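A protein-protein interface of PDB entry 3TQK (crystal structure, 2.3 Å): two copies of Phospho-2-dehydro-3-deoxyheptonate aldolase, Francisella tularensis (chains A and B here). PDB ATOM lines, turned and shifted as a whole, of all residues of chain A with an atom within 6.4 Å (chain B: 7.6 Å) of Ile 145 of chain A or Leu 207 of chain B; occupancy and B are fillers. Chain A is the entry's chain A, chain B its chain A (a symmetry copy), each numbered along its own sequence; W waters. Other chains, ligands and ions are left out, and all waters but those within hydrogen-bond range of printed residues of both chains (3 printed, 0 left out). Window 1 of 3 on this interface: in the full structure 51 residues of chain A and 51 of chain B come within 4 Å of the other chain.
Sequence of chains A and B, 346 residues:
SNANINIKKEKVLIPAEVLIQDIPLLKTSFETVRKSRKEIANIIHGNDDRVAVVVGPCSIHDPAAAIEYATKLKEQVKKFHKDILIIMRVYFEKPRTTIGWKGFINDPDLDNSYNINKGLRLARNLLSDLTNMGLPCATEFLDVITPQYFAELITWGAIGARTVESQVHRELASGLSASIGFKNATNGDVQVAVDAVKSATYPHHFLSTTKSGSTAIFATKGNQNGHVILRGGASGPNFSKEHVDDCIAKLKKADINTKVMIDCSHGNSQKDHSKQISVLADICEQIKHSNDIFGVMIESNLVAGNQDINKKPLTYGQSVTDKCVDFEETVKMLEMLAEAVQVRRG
OD1 of Asp 143 of chain A lies within hydrogen-bond range of N of Ile 145 of chain A. The side-chain carboxylate of Asp 143 of chain A is in hydrogen-bond range of the side-chain hydroxyl of Thr 146 of chain A (2.8 Å). O of Val 144 of chain A lies within hydrogen-bond range of OG of Ser 208 of chain A, at 3.4 Å. The side-chain hydroxyl (OG1) of Thr 209 of chain A sits at hydrogen-bond distance from the backbone carbonyl oxygen (O) of Val 144 of chain A (2.7 Å). O of Thr 209 of chain A lies within hydrogen-bond range of NE2 of Gln 148 of chain A (2.7 Å). The backbone carbonyl oxygen (O) of Ala 216 of chain B sits at hydrogen-bond distance from the backbone NH (N) of Ser 208 of chain B, 3.0 Å away.
CD2 of Leu 13 of chain A touches CD2 of Leu 207 of chain B, at 3.7 Å. OG1 of Thr 215 of chain B touches CD2 of Leu 13 of chain A (3.7 Å). CA of Ala 216 of chain B touches CB of Leu 13 of chain A (3.8 Å). CD2 of Leu 207 of chain B touches CG2 of Ile 116 of chain A (3.9 Å). Ile 116 of chain A touches Ile 217 of chain B. CD1 of Ile 145 of chain A touches C of Leu 207 of chain B (3.6 Å). CD1 of Ile 145 of chain A touches O of Ser 208 of chain B, 3.6 Å away. CG2 of Thr 146 of chain A touches CD1 of Leu 207 of chain B, 3.4 Å away. Ile 145 of chain B touches Ser 208 of chain A. Thr 209 of chain A touches Thr 215 of chain B (CG2 to CG2, 3.5 Å).
Of the printed residues of chain B, Leu 13 of chain A touches Leu 207 (3.7 Å), Thr 215 (3.7 Å) and Ala 216 (3.8 Å). Ile 145 of chain A touches two residues of chain B. Printed residues of chain B within 4 Å of Thr 146 of chain A: Leu 207 (3.4 Å). Printed residues of chain B within 4 Å of Ser 208 of chain A: Ile 145 (3.6 Å). Printed residues of chain B within 4 Å of Thr 209 of chain A: Thr 215 (3.5 Å). Of chain A, only Leu 13, Ile 116, Ile 145 and Thr 146 come within 4 Å of Leu 207 of chain B. Printed residues of chain A within 4 Å of Ile 217 of chain B: Ile 116 (3.7 Å).
Printed residues of chain B that touch a printed residue of chain A: Ile 145, Leu 207, Ser 208, Thr 215, Ala 216 and Ile 217. Among the printed residues, 10 pairs touch across the chains.
Ile 145 of chain A touches Ser 208 of chain B, and with the chains exchanged Ser 208 of chain A touches Ile 145 of chain B. Positions printed for both chains: 144, 145, 208 and 209. Of the 10 pairs that touch across the chains among the printed residues, 2 have their exchanged pair printed and touching as well.
Water W1 bridges the side-chain hydroxyl of Thr 215 of chain B (2.7 Å) and the side-chain hydroxyl of Tyr 149 of chain A (2.7 Å). Water W2 lies within hydrogen-bond range of the backbone carbonyl oxygen of Thr 215 of chain B (2.7 Å) and the backbone NH of Leu 13 of chain A (3.1 Å). Water W3 bridges the side-chain carboxylate of Asp 143 of chain A (2.8 Å) and the backbone carbonyl oxygen of Leu 207 of chain B (3.1 Å).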
ATOM      1  N   LEU A  13      -1.041 -16.131 -11.306  1.00  0.00           N
ATOM      2  CA  LEU A  13      -1.932 -15.760 -12.403  1.00  0.00           C
ATOM      3  C   LEU A  13      -1.821 -14.244 -12.618  1.00  0.00           C
ATOM      4  O   LEU A  13      -1.906 -13.482 -11.660  1.00  0.00           O
ATOM      5  CB  LEU A  13      -3.370 -16.125 -12.058  1.00  0.00           C
ATOM      6  CG  LEU A  13      -4.400 -15.922 -13.171  1.00  0.00           C
ATOM      7  CD1 LEU A  13      -4.120 -16.827 -14.359  1.00  0.00           C
ATOM      8  CD2 LEU A  13      -5.820 -16.159 -12.642  1.00  0.00           C
ATOM      9  N   ALA A  16      -6.356  -9.577 -15.112  1.00  0.00           N
ATOM     10  CA  ALA A  16      -6.905  -9.109 -16.387  1.00  0.00           C
ATOM     11  C   ALA A  16      -6.452  -7.701 -16.694  1.00  0.00           C
ATOM     12  O   ALA A  16      -6.218  -7.365 -17.856  1.00  0.00           O
ATOM     13  CB  ALA A  16      -8.436  -9.192 -16.378  1.00  0.00           C
ATOM     14  N   ILE A 105      -7.411 -22.277 -23.330  1.00  0.00           N
ATOM     15  CA  ILE A 105      -7.046 -21.514 -22.136  1.00  0.00           C
ATOM     16  C   ILE A 105      -6.265 -22.379 -21.139  1.00  0.00           C
ATOM     17  O   ILE A 105      -5.248 -21.950 -20.610  1.00  0.00           O
ATOM     18  CB  ILE A 105      -8.290 -20.853 -21.478  1.00  0.00           C
ATOM     19  CG1 ILE A 105      -8.746 -19.668 -22.338  1.00  0.00           C
ATOM     20  CG2 ILE A 105      -7.988 -20.386 -20.074  1.00  0.00           C
ATOM     21  CD1 ILE A 105     -10.091 -19.047 -21.898  1.00  0.00           C
ATOM     22  N   ILE A 116      -1.685 -21.443 -18.418  1.00  0.00           N
ATOM     23  CA  ILE A 116      -2.961 -20.770 -18.433  1.00  0.00           C
ATOM     24  C   ILE A 116      -2.781 -19.288 -18.705  1.00  0.00           C
ATOM     25  O   ILE A 116      -3.577 -18.703 -19.409  1.00  0.00           O
ATOM     26  CB  ILE A 116      -3.783 -21.022 -17.143  1.00  0.00           C
ATOM     27  CG1 ILE A 116      -4.058 -22.523 -16.986  1.00  0.00           C
ATOM     28  CG2 ILE A 116      -5.111 -20.257 -17.190  1.00  0.00           C
ATOM     29  CD1 ILE A 116      -4.611 -22.937 -15.630  1.00  0.00           C
ATOM     30  N   LEU A 120      -4.757 -17.380 -21.653  1.00  0.00           N
ATOM     31  CA  LEU A 120      -5.634 -16.238 -21.469  1.00  0.00           C
ATOM     32  C   LEU A 120      -5.177 -15.097 -22.347  1.00  0.00           C
ATOM     33  O   LEU A 120      -5.996 -14.415 -22.939  1.00  0.00           O
ATOM     34  CB  LEU A 120      -5.690 -15.787 -20.002  1.00  0.00           C
ATOM     35  CG  LEU A 120      -6.543 -16.663 -19.093  1.00  0.00           C
ATOM     36  CD1 LEU A 120      -6.225 -16.416 -17.601  1.00  0.00           C
ATOM     37  CD2 LEU A 120      -8.009 -16.426 -19.403  1.00  0.00           C
ATOM     38  N   ASP A 143     -16.615 -19.663 -15.793  1.00  0.00           N
ATOM     39  CA  ASP A 143     -16.356 -19.485 -14.355  1.00  0.00           C
ATOM     40  C   ASP A 143     -16.305 -17.998 -13.986  1.00  0.00           C
ATOM     41  O   ASP A 143     -16.594 -17.154 -14.835  1.00  0.00           O
ATOM     42  CB  ASP A 143     -15.066 -20.204 -13.985  1.00  0.00           C
ATOM     43  CG  ASP A 143     -13.820 -19.501 -14.507  1.00  0.00           C
ATOM     44  OD1 ASP A 143     -13.934 -18.527 -15.248  1.00  0.00           O
ATOM     45  OD2 ASP A 143     -12.701 -19.914 -14.151  1.00  0.00           O
ATOM     46  N   VAL A 144     -15.955 -17.662 -12.738  1.00  0.00           N
ATOM     47  CA  VAL A 144     -15.973 -16.255 -12.297  1.00  0.00           C
ATOM     48  C   VAL A 144     -14.632 -15.540 -12.462  1.00  0.00           C
ATOM     49  O   VAL A 144     -14.478 -14.397 -12.016  1.00  0.00           O
ATOM     50  CB  VAL A 144     -16.454 -16.116 -10.818  1.00  0.00           C
ATOM     51  CG1 VAL A 144     -17.864 -16.690 -10.655  1.00  0.00           C
ATOM     52  CG2 VAL A 144     -15.479 -16.762  -9.829  1.00  0.00           C
ATOM     53  N   ILE A 145     -13.669 -16.194 -13.111  1.00  0.00           N
ATOM     54  CA  ILE A 145     -12.314 -15.653 -13.230  1.00  0.00           C
ATOM     55  C   ILE A 145     -12.000 -15.272 -14.685  1.00  0.00           C
ATOM     56  O   ILE A 145     -11.610 -14.137 -14.954  1.00  0.00           O
ATOM     57  CB  ILE A 145     -11.269 -16.646 -12.641  1.00  0.00           C
ATOM     58  CG1 ILE A 145     -11.473 -16.759 -11.121  1.00  0.00           C
ATOM     59  CG2 ILE A 145      -9.858 -16.196 -12.926  1.00  0.00           C
ATOM     60  CD1 ILE A 145     -10.644 -17.869 -10.420  1.00  0.00           C
ATOM     61  N   THR A 146     -12.203 -16.200 -15.621  1.00  0.00           N
ATOM     62  CA  THR A 146     -11.821 -15.977 -17.018  1.00  0.00           C
ATOM     63  C   THR A 146     -12.558 -14.824 -17.701  1.00  0.00           C
ATOM     64  O   THR A 146     -11.956 -14.108 -18.492  1.00  0.00           O
ATOM     65  CB  THR A 146     -11.943 -17.267 -17.887  1.00  0.00           C
ATOM     66  OG1 THR A 146     -13.289 -17.762 -17.853  1.00  0.00           O
ATOM     67  CG2 THR A 146     -10.994 -18.366 -17.376  1.00  0.00           C
ATOM     68  N   PRO A 147     -13.847 -14.612 -17.392  1.00  0.00           N
ATOM     69  CA  PRO A 147     -14.556 -13.564 -18.131  1.00  0.00           C
ATOM     70  C   PRO A 147     -13.985 -12.158 -18.049  1.00  0.00           C
ATOM     71  O   PRO A 147     -14.133 -11.392 -18.995  1.00  0.00           O
ATOM     72  CB  PRO A 147     -15.948 -13.586 -17.503  1.00  0.00           C
ATOM     73  CG  PRO A 147     -16.102 -14.967 -17.007  1.00  0.00           C
ATOM     74  CD  PRO A 147     -14.761 -15.327 -16.481  1.00  0.00           C
ATOM     75  N   GLN A 148     -13.343 -11.809 -16.939  1.00  0.00           N
ATOM     76  CA  GLN A 148     -12.738 -10.487 -16.786  1.00  0.00           C
ATOM     77  C   GLN A 148     -11.657 -10.227 -17.826  1.00  0.00           C
ATOM     78  O   GLN A 148     -11.353  -9.074 -18.128  1.00  0.00           O
ATOM     79  CB  GLN A 148     -12.147 -10.326 -15.382  1.00  0.00           C
ATOM     80  CG  GLN A 148     -13.200 -10.247 -14.273  1.00  0.00           C
ATOM     81  CD  GLN A 148     -13.970  -8.910 -14.245  1.00  0.00           C
ATOM     82  OE1 GLN A 148     -13.903  -8.093 -15.183  1.00  0.00           O
ATOM     83  NE2 GLN A 148     -14.703  -8.685 -13.157  1.00  0.00           N
ATOM     84  N   TYR A 149     -11.096 -11.296 -18.392  1.00  0.00           N
ATOM     85  CA  TYR A 149     -10.059 -11.172 -19.392  1.00  0.00           C
ATOM     86  C   TYR A 149     -10.552 -10.808 -20.788  1.00  0.00           C
ATOM     87  O   TYR A 149      -9.748 -10.383 -21.621  1.00  0.00           O
ATOM     88  CB  TYR A 149      -9.226 -12.462 -19.451  1.00  0.00           C
ATOM     89  CG  TYR A 149      -8.416 -12.678 -18.204  1.00  0.00           C
ATOM     90  CD1 TYR A 149      -9.000 -13.186 -17.056  1.00  0.00           C
ATOM     91  CD2 TYR A 149      -7.072 -12.339 -18.163  1.00  0.00           C
ATOM     92  CE1 TYR A 149      -8.269 -13.367 -15.896  1.00  0.00           C
ATOM     93  CE2 TYR A 149      -6.314 -12.522 -17.002  1.00  0.00           C
ATOM     94  CZ  TYR A 149      -6.922 -13.030 -15.877  1.00  0.00           C
ATOM     95  OH  TYR A 149      -6.196 -13.217 -14.736  1.00  0.00           O
ATOM     96  N   SER A 208     -17.305 -12.919  -6.927  1.00  0.00           N
ATOM     97  CA  SER A 208     -16.643 -12.980  -8.223  1.00  0.00           C
ATOM     98  C   SER A 208     -15.272 -12.362  -8.070  1.00  0.00           C
ATOM     99  O   SER A 208     -14.774 -12.248  -6.951  1.00  0.00           O
ATOM    100  CB  SER A 208     -17.448 -12.242  -9.293  1.00  0.00           C
ATOM    101  OG  SER A 208     -16.975 -12.556 -10.605  1.00  0.00           O
ATOM    102  N   THR A 209     -14.656 -11.981  -9.185  1.00  0.00           N
ATOM    103  CA  THR A 209     -13.308 -11.435  -9.162  1.00  0.00           C
ATOM    104  C   THR A 209     -13.224 -10.155  -9.994  1.00  0.00           C
ATOM    105  O   THR A 209     -13.989  -9.972 -10.946  1.00  0.00           O
ATOM    106  CB  THR A 209     -12.234 -12.478  -9.640  1.00  0.00           C
ATOM    107  OG1 THR A 209     -12.461 -12.836 -11.013  1.00  0.00           O
ATOM    108  CG2 THR A 209     -12.274 -13.746  -8.763  1.00  0.00           C
ATOM    109  N   THR A 210     -12.301  -9.277  -9.606  1.00  0.00           N
ATOM    110  CA  THR A 210     -12.098  -7.989 -10.251  1.00  0.00           C
ATOM    111  C   THR A 210     -11.028  -8.069 -11.340  1.00  0.00           C
ATOM    112  O   THR A 210     -10.312  -9.058 -11.468  1.00  0.00           O
ATOM    113  CB  THR A 210     -11.604  -6.951  -9.238  1.00  0.00           C
ATOM    114  OG1 THR A 210     -10.297  -7.333  -8.799  1.00  0.00           O
ATOM    115  CG2 THR A 210     -12.549  -6.829  -8.032  1.00  0.00           C
ATOM    116  N   VAL B 144     -15.352 -21.340  -5.820  1.00  0.00           N
ATOM    117  CA  VAL B 144     -13.892 -21.301  -5.619  1.00  0.00           C
ATOM    118  C   VAL B 144     -13.430 -20.212  -4.652  1.00  0.00           C
ATOM    119  O   VAL B 144     -12.225 -19.991  -4.492  1.00  0.00           O
ATOM    120  CB  VAL B 144     -13.123 -21.151  -6.970  1.00  0.00           C
ATOM    121  CG1 VAL B 144     -13.450 -22.318  -7.906  1.00  0.00           C
ATOM    122  CG2 VAL B 144     -13.400 -19.806  -7.648  1.00  0.00           C
ATOM    123  N   ILE B 145     -14.378 -19.540  -3.995  1.00  0.00           N
ATOM    124  CA  ILE B 145     -14.058 -18.404  -3.130  1.00  0.00           C
ATOM    125  C   ILE B 145     -14.329 -18.741  -1.656  1.00  0.00           C
ATOM    126  O   ILE B 145     -13.441 -18.596  -0.818  1.00  0.00           O
ATOM    127  CB  ILE B 145     -14.819 -17.127  -3.593  1.00  0.00           C
ATOM    128  CG1 ILE B 145     -14.288 -16.685  -4.967  1.00  0.00           C
ATOM    129  CG2 ILE B 145     -14.655 -15.998  -2.605  1.00  0.00           C
ATOM    130  CD1 ILE B 145     -15.091 -15.550  -5.656  1.00  0.00           C
ATOM    131  N   VAL B 168     -15.604 -27.151 -12.732  1.00  0.00           N
ATOM    132  CA  VAL B 168     -14.789 -26.498 -11.704  1.00  0.00           C
ATOM    133  C   VAL B 168     -15.054 -27.130 -10.336  1.00  0.00           C
ATOM    134  O   VAL B 168     -14.179 -27.117  -9.473  1.00  0.00           O
ATOM    135  CB  VAL B 168     -14.979 -24.954 -11.651  1.00  0.00           C
ATOM    136  CG1 VAL B 168     -14.008 -24.310 -10.620  1.00  0.00           C
ATOM    137  CG2 VAL B 168     -14.726 -24.337 -13.035  1.00  0.00           C
ATOM    138  N   GLU B 171     -12.913 -30.189 -10.202  1.00  0.00           N
ATOM    139  CA  GLU B 171     -11.546 -29.697 -10.003  1.00  0.00           C
ATOM    140  C   GLU B 171     -11.298 -29.232  -8.574  1.00  0.00           C
ATOM    141  O   GLU B 171     -10.265 -29.552  -7.960  1.00  0.00           O
ATOM    142  CB  GLU B 171     -11.294 -28.549 -10.962  1.00  0.00           C
ATOM    143  CG  GLU B 171     -11.308 -28.991 -12.430  1.00  0.00           C
ATOM    144  CD  GLU B 171     -11.328 -27.842 -13.402  1.00  0.00           C
ATOM    145  OE1 GLU B 171     -11.692 -26.707 -13.034  1.00  0.00           O
ATOM    146  OE2 GLU B 171     -10.977 -28.082 -14.561  1.00  0.00           O
ATOM    147  N   LEU B 172     -12.253 -28.463  -8.066  1.00  0.00           N
ATOM    148  CA  LEU B 172     -12.249 -27.982  -6.692  1.00  0.00           C
ATOM    149  C   LEU B 172     -12.148 -29.150  -5.711  1.00  0.00           C
ATOM    150  O   LEU B 172     -11.342 -29.125  -4.788  1.00  0.00           O
ATOM    151  CB  LEU B 172     -13.532 -27.174  -6.427  1.00  0.00           C
ATOM    152  CG  LEU B 172     -13.870 -26.835  -4.983  1.00  0.00           C
ATOM    153  CD1 LEU B 172     -12.846 -25.830  -4.425  1.00  0.00           C
ATOM    154  CD2 LEU B 172     -15.265 -26.269  -4.894  1.00  0.00           C
ATOM    155  N   HIS B 205      -5.159 -28.710 -13.090  1.00  0.00           N
ATOM    156  CA  HIS B 205      -4.796 -27.305 -13.015  1.00  0.00           C
ATOM    157  C   HIS B 205      -6.079 -26.510 -13.244  1.00  0.00           C
ATOM    158  O   HIS B 205      -6.771 -26.726 -14.233  1.00  0.00           O
ATOM    159  CB  HIS B 205      -3.749 -26.952 -14.075  1.00  0.00           C
ATOM    160  CG  HIS B 205      -2.354 -27.364 -13.721  1.00  0.00           C
ATOM    161  ND1 HIS B 205      -1.972 -28.684 -13.599  1.00  0.00           N
ATOM    162  CD2 HIS B 205      -1.240 -26.628 -13.490  1.00  0.00           C
ATOM    163  CE1 HIS B 205      -0.687 -28.744 -13.299  1.00  0.00           C
ATOM    164  NE2 HIS B 205      -0.215 -27.511 -13.241  1.00  0.00           N
ATOM    165  N   PHE B 206      -6.418 -25.617 -12.320  1.00  0.00           N
ATOM    166  CA  PHE B 206      -7.615 -24.785 -12.476  1.00  0.00           C
ATOM    167  C   PHE B 206      -7.483 -23.453 -11.766  1.00  0.00           C
ATOM    168  O   PHE B 206      -6.632 -23.291 -10.904  1.00  0.00           O
ATOM    169  CB  PHE B 206      -8.854 -25.528 -11.978  1.00  0.00           C
ATOM    170  CG  PHE B 206      -9.020 -25.554 -10.470  1.00  0.00           C
ATOM    171  CD1 PHE B 206      -8.195 -26.320  -9.669  1.00  0.00           C
ATOM    172  CD2 PHE B 206     -10.050 -24.860  -9.867  1.00  0.00           C
ATOM    173  CE1 PHE B 206      -8.380 -26.359  -8.296  1.00  0.00           C
ATOM    174  CE2 PHE B 206     -10.244 -24.909  -8.508  1.00  0.00           C
ATOM    175  CZ  PHE B 206      -9.403 -25.655  -7.722  1.00  0.00           C
ATOM    176  N   LEU B 207      -8.343 -22.508 -12.137  1.00  0.00           N
ATOM    177  CA  LEU B 207      -8.346 -21.192 -11.557  1.00  0.00           C
ATOM    178  C   LEU B 207      -9.166 -21.163 -10.270  1.00  0.00           C
ATOM    179  O   LEU B 207     -10.315 -21.640 -10.237  1.00  0.00           O
ATOM    180  CB  LEU B 207      -8.879 -20.202 -12.572  1.00  0.00           C
ATOM    181  CG  LEU B 207      -8.063 -20.155 -13.866  1.00  0.00           C
ATOM    182  CD1 LEU B 207      -8.790 -19.322 -14.922  1.00  0.00           C
ATOM    183  CD2 LEU B 207      -6.655 -19.628 -13.612  1.00  0.00           C
ATOM    184  N   SER B 208      -8.562 -20.631  -9.208  1.00  0.00           N
ATOM    185  CA  SER B 208      -9.203 -20.548  -7.902  1.00  0.00           C
ATOM    186  C   SER B 208      -8.704 -19.294  -7.223  1.00  0.00           C
ATOM    187  O   SER B 208      -8.193 -18.398  -7.892  1.00  0.00           O
ATOM    188  CB  SER B 208      -8.889 -21.780  -7.051  1.00  0.00           C
ATOM    189  OG  SER B 208      -9.750 -21.854  -5.912  1.00  0.00           O
ATOM    190  N   THR B 209      -8.865 -19.219  -5.905  1.00  0.00           N
ATOM    191  CA  THR B 209      -8.482 -18.032  -5.157  1.00  0.00           C
ATOM    192  C   THR B 209      -7.662 -18.405  -3.922  1.00  0.00           C
ATOM    193  O   THR B 209      -7.811 -19.503  -3.377  1.00  0.00           O
ATOM    194  CB  THR B 209      -9.724 -17.156  -4.754  1.00  0.00           C
ATOM    195  OG1 THR B 209     -10.584 -17.887  -3.865  1.00  0.00           O
ATOM    196  CG2 THR B 209     -10.519 -16.725  -6.003  1.00  0.00           C
ATOM    197  N   SER B 214      -6.643 -13.239  -3.638  1.00  0.00           N
ATOM    198  CA  SER B 214      -6.156 -13.108  -4.997  1.00  0.00           C
ATOM    199  C   SER B 214      -6.584 -14.287  -5.848  1.00  0.00           C
ATOM    200  O   SER B 214      -6.865 -15.344  -5.323  1.00  0.00           O
ATOM    201  CB  SER B 214      -4.628 -13.055  -4.989  1.00  0.00           C
ATOM    202  OG  SER B 214      -4.123 -13.215  -6.314  1.00  0.00           O
ATOM    203  N   THR B 215      -6.608 -14.098  -7.166  1.00  0.00           N
ATOM    204  CA  THR B 215      -6.816 -15.202  -8.085  1.00  0.00           C
ATOM    205  C   THR B 215      -5.462 -15.884  -8.299  1.00  0.00           C
ATOM    206  O   THR B 215      -4.425 -15.252  -8.124  1.00  0.00           O
ATOM    207  CB  THR B 215      -7.403 -14.741  -9.446  1.00  0.00           C
ATOM    208  OG1 THR B 215      -6.578 -13.723 -10.014  1.00  0.00           O
ATOM    209  CG2 THR B 215      -8.825 -14.196  -9.295  1.00  0.00           C
ATOM    210  N   ALA B 216      -5.482 -17.164  -8.658  1.00  0.00           N
ATOM    211  CA  ALA B 216      -4.272 -17.959  -8.838  1.00  0.00           C
ATOM    212  C   ALA B 216      -4.583 -19.218  -9.610  1.00  0.00           C
ATOM    213  O   ALA B 216      -5.745 -19.626  -9.682  1.00  0.00           O
ATOM    214  CB  ALA B 216      -3.679 -18.344  -7.483  1.00  0.00           C
ATOM    215  N   ILE B 217      -3.544 -19.844 -10.170  1.00  0.00           N
ATOM    216  CA  ILE B 217      -3.666 -21.188 -10.738  1.00  0.00           C
ATOM    217  C   ILE B 217      -3.373 -22.196  -9.621  1.00  0.00           C
ATOM    218  O   ILE B 217      -2.383 -22.046  -8.896  1.00  0.00           O
ATOM    219  CB  ILE B 217      -2.670 -21.400 -11.899  1.00  0.00           C
ATOM    220  CG1 ILE B 217      -2.997 -20.481 -13.076  1.00  0.00           C
ATOM    221  CG2 ILE B 217      -2.646 -22.860 -12.359  1.00  0.00           C
ATOM    222  CD1 ILE B 217      -1.816 -20.294 -14.044  1.00  0.00           C
ATOM    223  N   PHE B 218      -4.229 -23.206  -9.470  1.00  0.00           N
ATOM    224  CA  PHE B 218      -4.014 -24.265  -8.487  1.00  0.00           C
ATOM    225  C   PHE B 218      -3.724 -25.594  -9.205  1.00  0.00           C
ATOM    226  O   PHE B 218      -4.507 -26.019 -10.050  1.00  0.00           O
ATOM    227  CB  PHE B 218      -5.256 -24.436  -7.602  1.00  0.00           C
ATOM    228  CG  PHE B 218      -5.356 -23.471  -6.433  1.00  0.00           C
ATOM    229  CD1 PHE B 218      -4.695 -22.258  -6.413  1.00  0.00           C
ATOM    230  CD2 PHE B 218      -6.183 -23.788  -5.358  1.00  0.00           C
ATOM    231  CE1 PHE B 218      -4.817 -21.382  -5.326  1.00  0.00           C
ATOM    232  CE2 PHE B 218      -6.325 -22.926  -4.275  1.00  0.00           C
ATOM    233  CZ  PHE B 218      -5.625 -21.705  -4.267  1.00  0.00           C
ATOM    234  N   ALA B 219      -2.589 -26.219  -8.890  1.00  0.00           N
ATOM    235  CA  ALA B 219      -2.291 -27.578  -9.309  1.00  0.00           C
ATOM    236  C   ALA B 219      -2.645 -28.518  -8.173  1.00  0.00           C
ATOM    237  O   ALA B 219      -2.028 -28.464  -7.105  1.00  0.00           O
ATOM    238  CB  ALA B 219      -0.795 -27.740  -9.690  1.00  0.00           C
HETATM  239  O   HOH W   1      -7.318 -12.655 -12.342  1.00  0.00           O
HETATM  240  O   HOH W   2      -1.756 -15.303  -8.431  1.00  0.00           O
HETATM  241  O   HOH W   3     -12.912 -20.392 -11.433  1.00  0.00           O
